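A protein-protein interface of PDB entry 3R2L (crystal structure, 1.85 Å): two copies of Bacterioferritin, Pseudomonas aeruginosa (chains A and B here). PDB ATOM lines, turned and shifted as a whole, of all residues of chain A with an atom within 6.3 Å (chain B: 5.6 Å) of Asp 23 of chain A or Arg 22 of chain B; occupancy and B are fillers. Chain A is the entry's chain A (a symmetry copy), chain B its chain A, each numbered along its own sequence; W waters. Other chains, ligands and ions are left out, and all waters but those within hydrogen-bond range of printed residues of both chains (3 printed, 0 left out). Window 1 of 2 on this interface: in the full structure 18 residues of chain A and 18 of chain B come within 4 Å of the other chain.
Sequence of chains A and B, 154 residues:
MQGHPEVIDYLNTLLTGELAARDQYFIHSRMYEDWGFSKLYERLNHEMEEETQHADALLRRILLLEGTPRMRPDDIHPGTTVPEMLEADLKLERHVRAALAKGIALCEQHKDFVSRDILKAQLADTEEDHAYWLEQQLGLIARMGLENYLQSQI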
ATOM      1  N   GLU A  18     -16.535 -31.772  13.644  1.00  0.00           N
ATOM      2  CA  GLU A  18     -17.785 -31.245  13.031  1.00  0.00           C
ATOM      3  C   GLU A  18     -18.776 -30.778  14.117  1.00  0.00           C
ATOM      4  O   GLU A  18     -19.444 -29.747  13.958  1.00  0.00           O
ATOM      5  CB  GLU A  18     -18.468 -32.314  12.127  1.00  0.00           C
ATOM      6  CG  GLU A  18     -17.580 -32.736  10.996  1.00  0.00           C
ATOM      7  CD  GLU A  18     -17.218 -31.564  10.100  1.00  0.00           C
ATOM      8  OE1 GLU A  18     -18.127 -30.874   9.644  1.00  0.00           O
ATOM      9  OE2 GLU A  18     -16.033 -31.312   9.858  1.00  0.00           O
ATOM     10  N   LEU A  19     -18.867 -31.522  15.209  1.00  0.00           N
ATOM     11  CA  LEU A  19     -19.682 -31.116  16.354  1.00  0.00           C
ATOM     12  C   LEU A  19     -19.210 -29.735  16.872  1.00  0.00           C
ATOM     13  O   LEU A  19     -20.014 -28.845  17.202  1.00  0.00           O
ATOM     14  CB  LEU A  19     -19.606 -32.177  17.465  1.00  0.00           C
ATOM     15  CG  LEU A  19     -20.217 -33.548  17.111  1.00  0.00           C
ATOM     16  CD1 LEU A  19     -19.923 -34.520  18.271  1.00  0.00           C
ATOM     17  CD2 LEU A  19     -21.744 -33.434  16.864  1.00  0.00           C
ATOM     18  N   ALA A  20     -17.892 -29.553  16.951  1.00  0.00           N
ATOM     19  CA  ALA A  20     -17.357 -28.252  17.284  1.00  0.00           C
ATOM     20  C   ALA A  20     -17.684 -27.147  16.251  1.00  0.00           C
ATOM     21  O   ALA A  20     -18.026 -26.023  16.639  1.00  0.00           O
ATOM     22  CB  ALA A  20     -15.813 -28.349  17.476  1.00  0.00           C
ATOM     23  N   ALA A  21     -17.511 -27.426  14.963  1.00  0.00           N
ATOM     24  CA  ALA A  21     -17.826 -26.430  13.914  1.00  0.00           C
ATOM     25  C   ALA A  21     -19.304 -25.984  14.074  1.00  0.00           C
ATOM     26  O   ALA A  21     -19.622 -24.778  14.042  1.00  0.00           O
ATOM     27  CB  ALA A  21     -17.642 -27.052  12.579  1.00  0.00           C
ATOM     28  N   ARG A  22     -20.182 -26.986  14.242  1.00  0.00           N
ATOM     29  CA  ARG A  22     -21.630 -26.750  14.475  1.00  0.00           C
ATOM     30  C   ARG A  22     -21.790 -25.750  15.649  1.00  0.00           C
ATOM     31  O   ARG A  22     -22.437 -24.715  15.532  1.00  0.00           O
ATOM     32  CB  ARG A  22     -22.295 -28.080  14.793  1.00  0.00           C
ATOM     33  CG  ARG A  22     -23.707 -27.948  15.400  1.00  0.00           C
ATOM     34  CD  ARG A  22     -24.133 -29.235  16.157  1.00  0.00           C
ATOM     35  NE  ARG A  22     -23.226 -29.557  17.280  1.00  0.00           N
ATOM     36  CZ  ARG A  22     -23.453 -30.494  18.199  1.00  0.00           C
ATOM     37  NH1 ARG A  22     -24.547 -31.266  18.143  1.00  0.00           N
ATOM     38  NH2 ARG A  22     -22.556 -30.691  19.161  1.00  0.00           N
ATOM     39  N   ASP A  23     -21.146 -26.032  16.772  1.00  0.00           N
ATOM     40  CA  ASP A  23     -21.237 -25.148  17.930  1.00  0.00           C
ATOM     41  C   ASP A  23     -20.614 -23.776  17.792  1.00  0.00           C
ATOM     42  O   ASP A  23     -21.171 -22.777  18.335  1.00  0.00           O
ATOM     43  CB  ASP A  23     -20.765 -25.866  19.216  1.00  0.00           C
ATOM     44  CG  ASP A  23     -21.742 -26.982  19.625  1.00  0.00           C
ATOM     45  OD1 ASP A  23     -22.886 -26.948  19.124  1.00  0.00           O
ATOM     46  OD2 ASP A  23     -21.398 -27.889  20.400  1.00  0.00           O
ATOM     47  N   GLN A  24     -19.534 -23.668  17.027  1.00  0.00           N
ATOM     48  CA  GLN A  24     -18.934 -22.353  16.851  1.00  0.00           C
ATOM     49  C   GLN A  24     -19.863 -21.499  15.955  1.00  0.00           C
ATOM     50  O   GLN A  24     -20.039 -20.310  16.180  1.00  0.00           O
ATOM     51  CB  GLN A  24     -17.532 -22.460  16.241  1.00  0.00           C
ATOM     52  CG  GLN A  24     -16.835 -21.125  16.152  1.00  0.00           C
ATOM     53  CD  GLN A  24     -15.323 -21.310  15.931  1.00  0.00           C
ATOM     54  OE1 GLN A  24     -14.741 -20.888  14.906  1.00  0.00           O
ATOM     55  NE2 GLN A  24     -14.711 -22.001  16.844  1.00  0.00           N
ATOM     56  N   TYR A  25     -20.461 -22.103  14.936  1.00  0.00           N
ATOM     57  CA  TYR A  25     -21.455 -21.368  14.124  1.00  0.00           C
ATOM     58  C   TYR A  25     -22.724 -21.042  14.930  1.00  0.00           C
ATOM     59  O   TYR A  25     -23.362 -19.998  14.700  1.00  0.00           O
ATOM     60  CB  TYR A  25     -21.839 -22.216  12.927  1.00  0.00           C
ATOM     61  CG  TYR A  25     -20.734 -22.268  11.869  1.00  0.00           C
ATOM     62  CD1 TYR A  25     -20.042 -21.112  11.519  1.00  0.00           C
ATOM     63  CD2 TYR A  25     -20.435 -23.435  11.202  1.00  0.00           C
ATOM     64  CE1 TYR A  25     -19.061 -21.113  10.488  1.00  0.00           C
ATOM     65  CE2 TYR A  25     -19.451 -23.459  10.197  1.00  0.00           C
ATOM     66  CZ  TYR A  25     -18.769 -22.290   9.844  1.00  0.00           C
ATOM     67  OH  TYR A  25     -17.793 -22.273   8.850  1.00  0.00           O
ATOM     68  N   PHE A  26     -23.062 -21.919  15.879  1.00  0.00           N
ATOM     69  CA  PHE A  26     -24.223 -21.691  16.799  1.00  0.00           C
ATOM     70  C   PHE A  26     -23.997 -20.352  17.526  1.00  0.00           C
ATOM     71  O   PHE A  26     -24.776 -19.385  17.428  1.00  0.00           O
ATOM     72  CB  PHE A  26     -24.334 -22.849  17.811  1.00  0.00           C
ATOM     73  CG  PHE A  26     -25.716 -23.020  18.484  1.00  0.00           C
ATOM     74  CD1 PHE A  26     -25.934 -24.127  19.302  1.00  0.00           C
ATOM     75  CD2 PHE A  26     -26.748 -22.088  18.328  1.00  0.00           C
ATOM     76  CE1 PHE A  26     -27.152 -24.350  19.944  1.00  0.00           C
ATOM     77  CE2 PHE A  26     -27.997 -22.285  18.952  1.00  0.00           C
ATOM     78  CZ  PHE A  26     -28.211 -23.419  19.766  1.00  0.00           C
ATOM     79  N   ILE A  27     -22.899 -20.260  18.262  1.00  0.00           N
ATOM     80  CA  ILE A  27     -22.636 -19.033  18.967  1.00  0.00           C
ATOM     81  C   ILE A  27     -22.368 -17.846  18.047  1.00  0.00           C
ATOM     82  O   ILE A  27     -22.899 -16.761  18.293  1.00  0.00           O
ATOM     83  CB  ILE A  27     -21.492 -19.198  20.037  1.00  0.00           C
ATOM     84  CG1 ILE A  27     -21.272 -17.886  20.790  1.00  0.00           C
ATOM     85  CG2 ILE A  27     -20.200 -19.660  19.389  1.00  0.00           C
ATOM     86  CD1 ILE A  27     -22.439 -17.489  21.656  1.00  0.00           C
ATOM     87  N   HIS A  28     -21.570 -17.985  16.989  1.00  0.00           N
ATOM     88  CA  HIS A  28     -21.338 -16.789  16.155  1.00  0.00           C
ATOM     89  C   HIS A  28     -22.627 -16.279  15.509  1.00  0.00           C
ATOM     90  O   HIS A  28     -22.821 -15.051  15.389  1.00  0.00           O
ATOM     91  CB  HIS A  28     -20.319 -17.039  15.039  1.00  0.00           C
ATOM     92  CG  HIS A  28     -18.878 -17.066  15.499  1.00  0.00           C
ATOM     93  ND1 HIS A  28     -17.868 -17.574  14.705  1.00  0.00           N
ATOM     94  CD2 HIS A  28     -18.273 -16.592  16.619  1.00  0.00           C
ATOM     95  CE1 HIS A  28     -16.703 -17.425  15.319  1.00  0.00           C
ATOM     96  NE2 HIS A  28     -16.918 -16.834  16.483  1.00  0.00           N
ATOM     97  N   MET A  48     -24.445 -23.746  10.540  1.00  0.00           N
ATOM     98  CA  MET A  48     -24.681 -24.644  11.688  1.00  0.00           C
ATOM     99  C   MET A  48     -25.495 -25.869  11.285  1.00  0.00           C
ATOM    100  O   MET A  48     -25.171 -27.022  11.681  1.00  0.00           O
ATOM    101  CB  MET A  48     -25.419 -23.917  12.817  1.00  0.00           C
ATOM    102  CG  MET A  48     -25.607 -24.785  14.028  1.00  0.00           C
ATOM    103  SD  MET A  48     -26.516 -23.988  15.354  1.00  0.00           S
ATOM    104  CE  MET A  48     -28.154 -23.755  14.622  1.00  0.00           C
ATOM    105  N   GLU A  51     -23.231 -28.175   9.229  1.00  0.00           N
ATOM    106  CA  GLU A  51     -22.259 -28.957  10.029  1.00  0.00           C
ATOM    107  C   GLU A  51     -22.975 -30.047  10.801  1.00  0.00           C
ATOM    108  O   GLU A  51     -22.416 -31.082  11.065  1.00  0.00           O
ATOM    109  CB  GLU A  51     -21.481 -28.084  11.039  1.00  0.00           C
ATOM    110  CG  GLU A  51     -20.747 -26.889  10.429  1.00  0.00           C
ATOM    111  CD  GLU A  51     -19.627 -27.260   9.434  1.00  0.00           C
ATOM    112  OE1 GLU A  51     -19.422 -28.423   9.109  1.00  0.00           O
ATOM    113  OE2 GLU A  51     -18.951 -26.352   8.981  1.00  0.00           O
ATOM    114  N   PRO A  73     -17.555 -32.575  21.654  1.00  0.00           N
ATOM    115  CA  PRO A  73     -17.013 -31.682  20.628  1.00  0.00           C
ATOM    116  C   PRO A  73     -15.610 -31.192  20.987  1.00  0.00           C
ATOM    117  O   PRO A  73     -15.319 -31.036  22.183  1.00  0.00           O
ATOM    118  CB  PRO A  73     -17.993 -30.477  20.621  1.00  0.00           C
ATOM    119  CG  PRO A  73     -19.271 -31.012  21.379  1.00  0.00           C
ATOM    120  CD  PRO A  73     -18.730 -32.015  22.357  1.00  0.00           C
ATOM    121  N   ILE A  76     -14.136 -24.929  21.059  1.00  0.00           N
ATOM    122  CA  ILE A  76     -14.285 -23.875  20.058  1.00  0.00           C
ATOM    123  C   ILE A  76     -13.575 -22.628  20.541  1.00  0.00           C
ATOM    124  O   ILE A  76     -13.207 -22.546  21.694  1.00  0.00           O
ATOM    125  CB  ILE A  76     -15.771 -23.539  19.802  1.00  0.00           C
ATOM    126  CG1 ILE A  76     -16.464 -23.132  21.107  1.00  0.00           C
ATOM    127  CG2 ILE A  76     -16.484 -24.764  19.166  1.00  0.00           C
ATOM    128  CD1 ILE A  76     -17.874 -22.502  20.855  1.00  0.00           C
ATOM    129  N   GLY B  17     -26.028 -27.849  29.957  1.00  0.00           N
ATOM    130  CA  GLY B  17     -26.866 -29.032  30.160  1.00  0.00           C
ATOM    131  C   GLY B  17     -27.778 -29.314  28.943  1.00  0.00           C
ATOM    132  O   GLY B  17     -27.983 -30.468  28.591  1.00  0.00           O
ATOM    133  N   GLU B  18     -28.342 -28.269  28.318  1.00  0.00           N
ATOM    134  CA  GLU B  18     -29.225 -28.465  27.136  1.00  0.00           C
ATOM    135  C   GLU B  18     -28.406 -28.905  25.905  1.00  0.00           C
ATOM    136  O   GLU B  18     -28.848 -29.764  25.129  1.00  0.00           O
ATOM    137  CB  GLU B  18     -30.018 -27.167  26.798  1.00  0.00           C
ATOM    138  CG  GLU B  18     -30.904 -26.746  27.930  1.00  0.00           C
ATOM    139  CD  GLU B  18     -31.928 -27.815  28.270  1.00  0.00           C
ATOM    140  OE1 GLU B  18     -32.635 -28.255  27.366  1.00  0.00           O
ATOM    141  OE2 GLU B  18     -32.025 -28.236  29.427  1.00  0.00           O
ATOM    142  N   LEU B  19     -27.227 -28.330  25.730  1.00  0.00           N
ATOM    143  CA  LEU B  19     -26.313 -28.752  24.668  1.00  0.00           C
ATOM    144  C   LEU B  19     -25.983 -30.256  24.825  1.00  0.00           C
ATOM    145  O   LEU B  19     -25.946 -31.028  23.849  1.00  0.00           O
ATOM    146  CB  LEU B  19     -25.032 -27.901  24.699  1.00  0.00           C
ATOM    147  CG  LEU B  19     -25.224 -26.405  24.376  1.00  0.00           C
ATOM    148  CD1 LEU B  19     -23.878 -25.687  24.597  1.00  0.00           C
ATOM    149  CD2 LEU B  19     -25.721 -26.205  22.921  1.00  0.00           C
ATOM    150  N   ALA B  20     -25.736 -30.681  26.063  1.00  0.00           N
ATOM    151  CA  ALA B  20     -25.562 -32.092  26.326  1.00  0.00           C
ATOM    152  C   ALA B  20     -26.814 -32.952  26.031  1.00  0.00           C
ATOM    153  O   ALA B  20     -26.691 -34.042  25.458  1.00  0.00           O
ATOM    154  CB  ALA B  20     -25.120 -32.303  27.807  1.00  0.00           C
ATOM    155  N   ALA B  21     -27.989 -32.518  26.476  1.00  0.00           N
ATOM    156  CA  ALA B  21     -29.234 -33.272  26.211  1.00  0.00           C
ATOM    157  C   ALA B  21     -29.388 -33.465  24.679  1.00  0.00           C
ATOM    158  O   ALA B  21     -29.683 -34.577  24.194  1.00  0.00           O
ATOM    159  CB  ALA B  21     -30.392 -32.499  26.727  1.00  0.00           C
ATOM    160  N   ARG B  22     -29.181 -32.360  23.945  1.00  0.00           N
ATOM    161  CA  ARG B  22     -29.220 -32.365  22.461  1.00  0.00           C
ATOM    162  C   ARG B  22     -28.283 -33.485  21.940  1.00  0.00           C
ATOM    163  O   ARG B  22     -28.682 -34.358  21.178  1.00  0.00           O
ATOM    164  CB  ARG B  22     -28.776 -31.001  21.956  1.00  0.00           C
ATOM    165  CG  ARG B  22     -28.428 -30.968  20.454  1.00  0.00           C
ATOM    166  CD  ARG B  22     -27.528 -29.754  20.096  1.00  0.00           C
ATOM    167  NE  ARG B  22     -26.239 -29.773  20.821  1.00  0.00           N
ATOM    168  CZ  ARG B  22     -25.214 -28.960  20.574  1.00  0.00           C
ATOM    169  NH1 ARG B  22     -25.300 -28.005  19.638  1.00  0.00           N
ATOM    170  NH2 ARG B  22     -24.105 -29.073  21.300  1.00  0.00           N
ATOM    171  N   ASP B  23     -27.042 -33.496  22.405  1.00  0.00           N
ATOM    172  CA  ASP B  23     -26.089 -34.513  21.972  1.00  0.00           C
ATOM    173  C   ASP B  23     -26.372 -35.937  22.396  1.00  0.00           C
ATOM    174  O   ASP B  23     -26.109 -36.891  21.605  1.00  0.00           O
ATOM    175  CB  ASP B  23     -24.638 -34.093  22.304  1.00  0.00           C
ATOM    176  CG  ASP B  23     -24.192 -32.895  21.448  1.00  0.00           C
ATOM    177  OD1 ASP B  23     -24.862 -32.647  20.422  1.00  0.00           O
ATOM    178  OD2 ASP B  23     -23.224 -32.191  21.778  1.00  0.00           O
ATOM    179  N   GLN B  24     -26.968 -36.120  23.569  1.00  0.00           N
ATOM    180  CA  GLN B  24     -27.281 -37.480  23.986  1.00  0.00           C
ATOM    181  C   GLN B  24     -28.448 -38.009  23.117  1.00  0.00           C
ATOM    182  O   GLN B  24     -28.469 -39.168  22.727  1.00  0.00           O
ATOM    183  CB  GLN B  24     -27.638 -37.535  25.475  1.00  0.00           C
ATOM    184  CG  GLN B  24     -27.855 -38.944  25.968  1.00  0.00           C
ATOM    185  CD  GLN B  24     -27.803 -39.001  27.505  1.00  0.00           C
ATOM    186  OE1 GLN B  24     -28.785 -39.362  28.194  1.00  0.00           O
ATOM    187  NE2 GLN B  24     -26.698 -38.576  28.037  1.00  0.00           N
ATOM    188  N   TYR B  25     -29.423 -37.162  22.813  1.00  0.00           N
ATOM    189  CA  TYR B  25     -30.497 -37.576  21.885  1.00  0.00           C
ATOM    190  C   TYR B  25     -29.968 -37.788  20.456  1.00  0.00           C
ATOM    191  O   TYR B  25     -30.477 -38.654  19.721  1.00  0.00           O
ATOM    192  CB  TYR B  25     -31.567 -36.503  21.857  1.00  0.00           C
ATOM    193  CG  TYR B  25     -32.415 -36.492  23.132  1.00  0.00           C
ATOM    194  CD1 TYR B  25     -32.855 -37.687  23.693  1.00  0.00           C
ATOM    195  CD2 TYR B  25     -32.808 -35.309  23.720  1.00  0.00           C
ATOM    196  CE1 TYR B  25     -33.705 -37.706  24.835  1.00  0.00           C
ATOM    197  CE2 TYR B  25     -33.629 -35.311  24.862  1.00  0.00           C
ATOM    198  CZ  TYR B  25     -34.075 -36.517  25.413  1.00  0.00           C
ATOM    199  OH  TYR B  25     -34.893 -36.557  26.540  1.00  0.00           O
ATOM    200  N   PHE B  26     -28.941 -37.017  20.086  1.00  0.00           N
ATOM    201  CA  PHE B  26     -28.267 -37.170  18.756  1.00  0.00           C
ATOM    202  C   PHE B  26     -27.765 -38.621  18.641  1.00  0.00           C
ATOM    203  O   PHE B  26     -28.154 -39.408  17.757  1.00  0.00           O
ATOM    204  CB  PHE B  26     -27.095 -36.177  18.638  1.00  0.00           C
ATOM    205  CG  PHE B  26     -26.624 -35.864  17.198  1.00  0.00           C
ATOM    206  CD1 PHE B  26     -25.665 -34.872  17.004  1.00  0.00           C
ATOM    207  CD2 PHE B  26     -27.101 -36.562  16.083  1.00  0.00           C
ATOM    208  CE1 PHE B  26     -25.189 -34.534  15.737  1.00  0.00           C
ATOM    209  CE2 PHE B  26     -26.653 -36.242  14.786  1.00  0.00           C
ATOM    210  CZ  PHE B  26     -25.692 -35.224  14.600  1.00  0.00           C
ATOM    211  N   ILE B  27     -26.897 -39.019  19.561  1.00  0.00           N
ATOM    212  CA  ILE B  27     -26.391 -40.364  19.503  1.00  0.00           C
ATOM    213  C   ILE B  27     -27.456 -41.428  19.752  1.00  0.00           C
ATOM    214  O   ILE B  27     -27.493 -42.426  19.028  1.00  0.00           O
ATOM    215  CB  ILE B  27     -25.145 -40.570  20.445  1.00  0.00           C
ATOM    216  CG1 ILE B  27     -24.614 -41.998  20.324  1.00  0.00           C
ATOM    217  CG2 ILE B  27     -25.492 -40.254  21.887  1.00  0.00           C
ATOM    218  CD1 ILE B  27     -24.024 -42.306  18.972  1.00  0.00           C
ATOM    219  N   MET B  48     -34.016 -34.190  19.991  1.00  0.00           N
ATOM    220  CA  MET B  48     -32.776 -33.448  19.687  1.00  0.00           C
ATOM    221  C   MET B  48     -33.074 -32.051  19.154  1.00  0.00           C
ATOM    222  O   MET B  48     -32.434 -31.047  19.570  1.00  0.00           O
ATOM    223  CB  MET B  48     -31.923 -34.193  18.654  1.00  0.00           C
ATOM    224  CG  MET B  48     -30.621 -33.497  18.382  1.00  0.00           C
ATOM    225  SD  MET B  48     -29.615 -34.309  17.137  1.00  0.00           S
ATOM    226  CE  MET B  48     -30.622 -34.133  15.644  1.00  0.00           C
ATOM    227  N   GLU B  51     -34.310 -29.903  22.075  1.00  0.00           N
ATOM    228  CA  GLU B  51     -33.243 -29.438  22.992  1.00  0.00           C
ATOM    229  C   GLU B  51     -32.408 -28.366  22.319  1.00  0.00           C
ATOM    230  O   GLU B  51     -31.880 -27.499  22.970  1.00  0.00           O
ATOM    231  CB  GLU B  51     -32.297 -30.578  23.432  1.00  0.00           C
ATOM    232  CG  GLU B  51     -32.990 -31.779  24.076  1.00  0.00           C
ATOM    233  CD  GLU B  51     -33.717 -31.469  25.402  1.00  0.00           C
ATOM    234  OE1 GLU B  51     -33.793 -30.325  25.836  1.00  0.00           O
ATOM    235  OE2 GLU B  51     -34.216 -32.404  26.005  1.00  0.00           O
ATOM    236  N   THR B  52     -32.220 -28.446  21.009  1.00  0.00           N
ATOM    237  CA  THR B  52     -31.477 -27.393  20.311  1.00  0.00           C
ATOM    238  C   THR B  52     -32.199 -26.048  20.454  1.00  0.00           C
ATOM    239  O   THR B  52     -31.577 -24.998  20.665  1.00  0.00           O
ATOM    240  CB  THR B  52     -31.267 -27.784  18.831  1.00  0.00           C
ATOM    241  OG1 THR B  52     -30.588 -29.054  18.782  1.00  0.00           O
ATOM    242  CG2 THR B  52     -30.468 -26.752  18.080  1.00  0.00           C
ATOM    243  N   MET B  71     -20.243 -22.581  25.760  1.00  0.00           N
ATOM    244  CA  MET B  71     -20.707 -23.493  24.689  1.00  0.00           C
ATOM    245  C   MET B  71     -20.200 -24.937  24.858  1.00  0.00           C
ATOM    246  O   MET B  71     -20.486 -25.798  24.045  1.00  0.00           O
ATOM    247  CB  MET B  71     -20.272 -22.965  23.319  1.00  0.00           C
ATOM    248  CG  MET B  71     -20.937 -21.621  22.904  1.00  0.00           C
ATOM    249  SD  MET B  71     -22.766 -21.698  22.923  1.00  0.00           S
ATOM    250  CE  MET B  71     -23.081 -22.875  21.607  1.00  0.00           C
ATOM    251  N   PRO B  73     -20.574 -28.511  25.988  1.00  0.00           N
ATOM    252  CA  PRO B  73     -21.646 -29.321  26.568  1.00  0.00           C
ATOM    253  C   PRO B  73     -21.168 -30.103  27.791  1.00  0.00           C
ATOM    254  O   PRO B  73     -19.989 -30.486  27.833  1.00  0.00           O
ATOM    255  CB  PRO B  73     -22.020 -30.317  25.435  1.00  0.00           C
ATOM    256  CG  PRO B  73     -21.385 -29.682  24.135  1.00  0.00           C
ATOM    257  CD  PRO B  73     -20.172 -28.951  24.634  1.00  0.00           C
HETATM  258  O   HOH W   1     -19.369 -27.095  21.724  1.00  0.00           O
HETATM  259  O   HOH W   2     -26.868 -26.959  17.407  1.00  0.00           O
HETATM  260  O   HOH W   3     -27.144 -31.667  16.868  1.00  0.00           O
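Leu 19 of chain A touches Phe 26 of chain B, and with the chains exchanged Phe 26 of chain A touches Leu 19 of chain B.
Arg 22 of chain A touches its own counterpart, Arg 22 of chain B.
Arg 22 of chain A touches Phe 26 of chain B, and with the chains exchanged Phe 26 of chain A touches Arg 22 of chain B.
Pro 73 of chain A touches its own counterpart, Pro 73 of chain B.
Of the 13 pairs that touch across the chains among the printed residues, 8 have their exchanged pair printed and touching as well.
Water W1 bridges OD2 of Asp 23 of chain A and O of Met 71 of chain B.
Water W2 bridges NH1 of Arg 22 of chain B and SD of Met 48 of chain A.
Water W3 lies within hydrogen-bond range of the guanidinium group of Arg 22 of chain A and the side-chain sulfur of Met 48 of chain B.
Among the printed residues, merely in contact across the chains: Ile 76 of chain A with Met 71 of chain B (3.5 Å), Pro 73 of chain A with Pro 73 of chain B (3.7 Å), Leu 19 of chain A with Phe 26 of chain B (3.8 Å), Phe 26 of chain A with Leu 19 of chain B (3.8 Å), Asp 23 of chain A with Met 71 of chain B (3.8 Å), Ile 27 of chain A with Met 71 of chain B (3.8 Å), Phe 26 of chain A with Thr 52 of chain B (3.8 Å), Phe 26 of chain A with Met 71 of chain B (3.9 Å), Arg 22 of chain A with Phe 26 of chain B (3.9 Å) and Phe 26 of chain A with Arg 22 of chain B (3.9 Å).
Hydrophobic or aromatic side chains of chain B that line the printed part of chain A: Leu 19, Phe 26, Met 71 and Pro 73.
Printed residues of chain A that touch a printed residue of chain B: Leu 19, Arg 22, Asp 23, Phe 26, Ile 27, Pro 73 and Ile 76.
Among the printed residues, 13 pairs touch across the chains.
Among the printed residues, Asp or Glu carboxylates within 4 Å of a Lys or Arg side-chain nitrogen of the other chain: Arg 22 of chain A with Asp 23 of chain B (2.7 Å) and Asp 23 of chain A with Arg 22 of chain B (2.7 Å).
Of the printed residues of chain B, Leu 19 of chain A touches Phe 26 (3.8 Å).
Of chain B, only Arg 22 (2.7 Å) and Met 71 (3.8 Å) come within 4 Å of Asp 23 of chain A.
Gln 24 of chain A touches none of the printed residues of chain B.
Printed residues of chain B within 4 Å of Phe 26 of chain A: Leu 19 (3.8 Å), Arg 22 (3.9 Å), Thr 52 (3.8 Å) and Met 71 (3.9 Å).
Of the printed residues of chain A, Leu 19 of chain B touches Phe 26 (3.8 Å).
Of the printed residues of chain A, Pro 73 of chain B touches Pro 73.
The nearest residue of chain B that does not touch Asp 23 of chain A is Pro 73 of chain B (4.1 Å).
The nearest residue of chain A that does not touch Arg 22 of chain B is Pro 73 of chain A (5.2 Å).
The backbone carbonyl oxygen (O) of Leu 19 of chain B lies within hydrogen-bond range of the guanidinium group (NE) of Arg 22 of chain B.
NE of Arg 22 of chain B lies within salt-bridge range of OD1 of Asp 23 of chain B, 3.2 Å away.
The side-chain hydroxyl (OG1) of Thr 52 of chain B sits at hydrogen-bond distance from the backbone carbonyl oxygen (O) of Met 48 of chain B, 2.8 Å away.
O of Leu 19 of chain A lies within hydrogen-bond range of NE of Arg 22 of chain A (3.3 Å).
The guanidinium group of Arg 22 of chain A is in salt-bridge range of the side-chain carboxylate of Asp 23 of chain A.
The guanidinium group of Arg 22 of chain B is in salt-bridge range of the side-chain carboxylate of Asp 23 of chain A, at 2.7 Å.
NH1 of Arg 22 of chain A is in salt-bridge range of OD1 of Asp 23 of chain B.
NH2 of Arg 22 of chain A sits close to NH2 of Arg 22 of chain B (3.1 Å).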
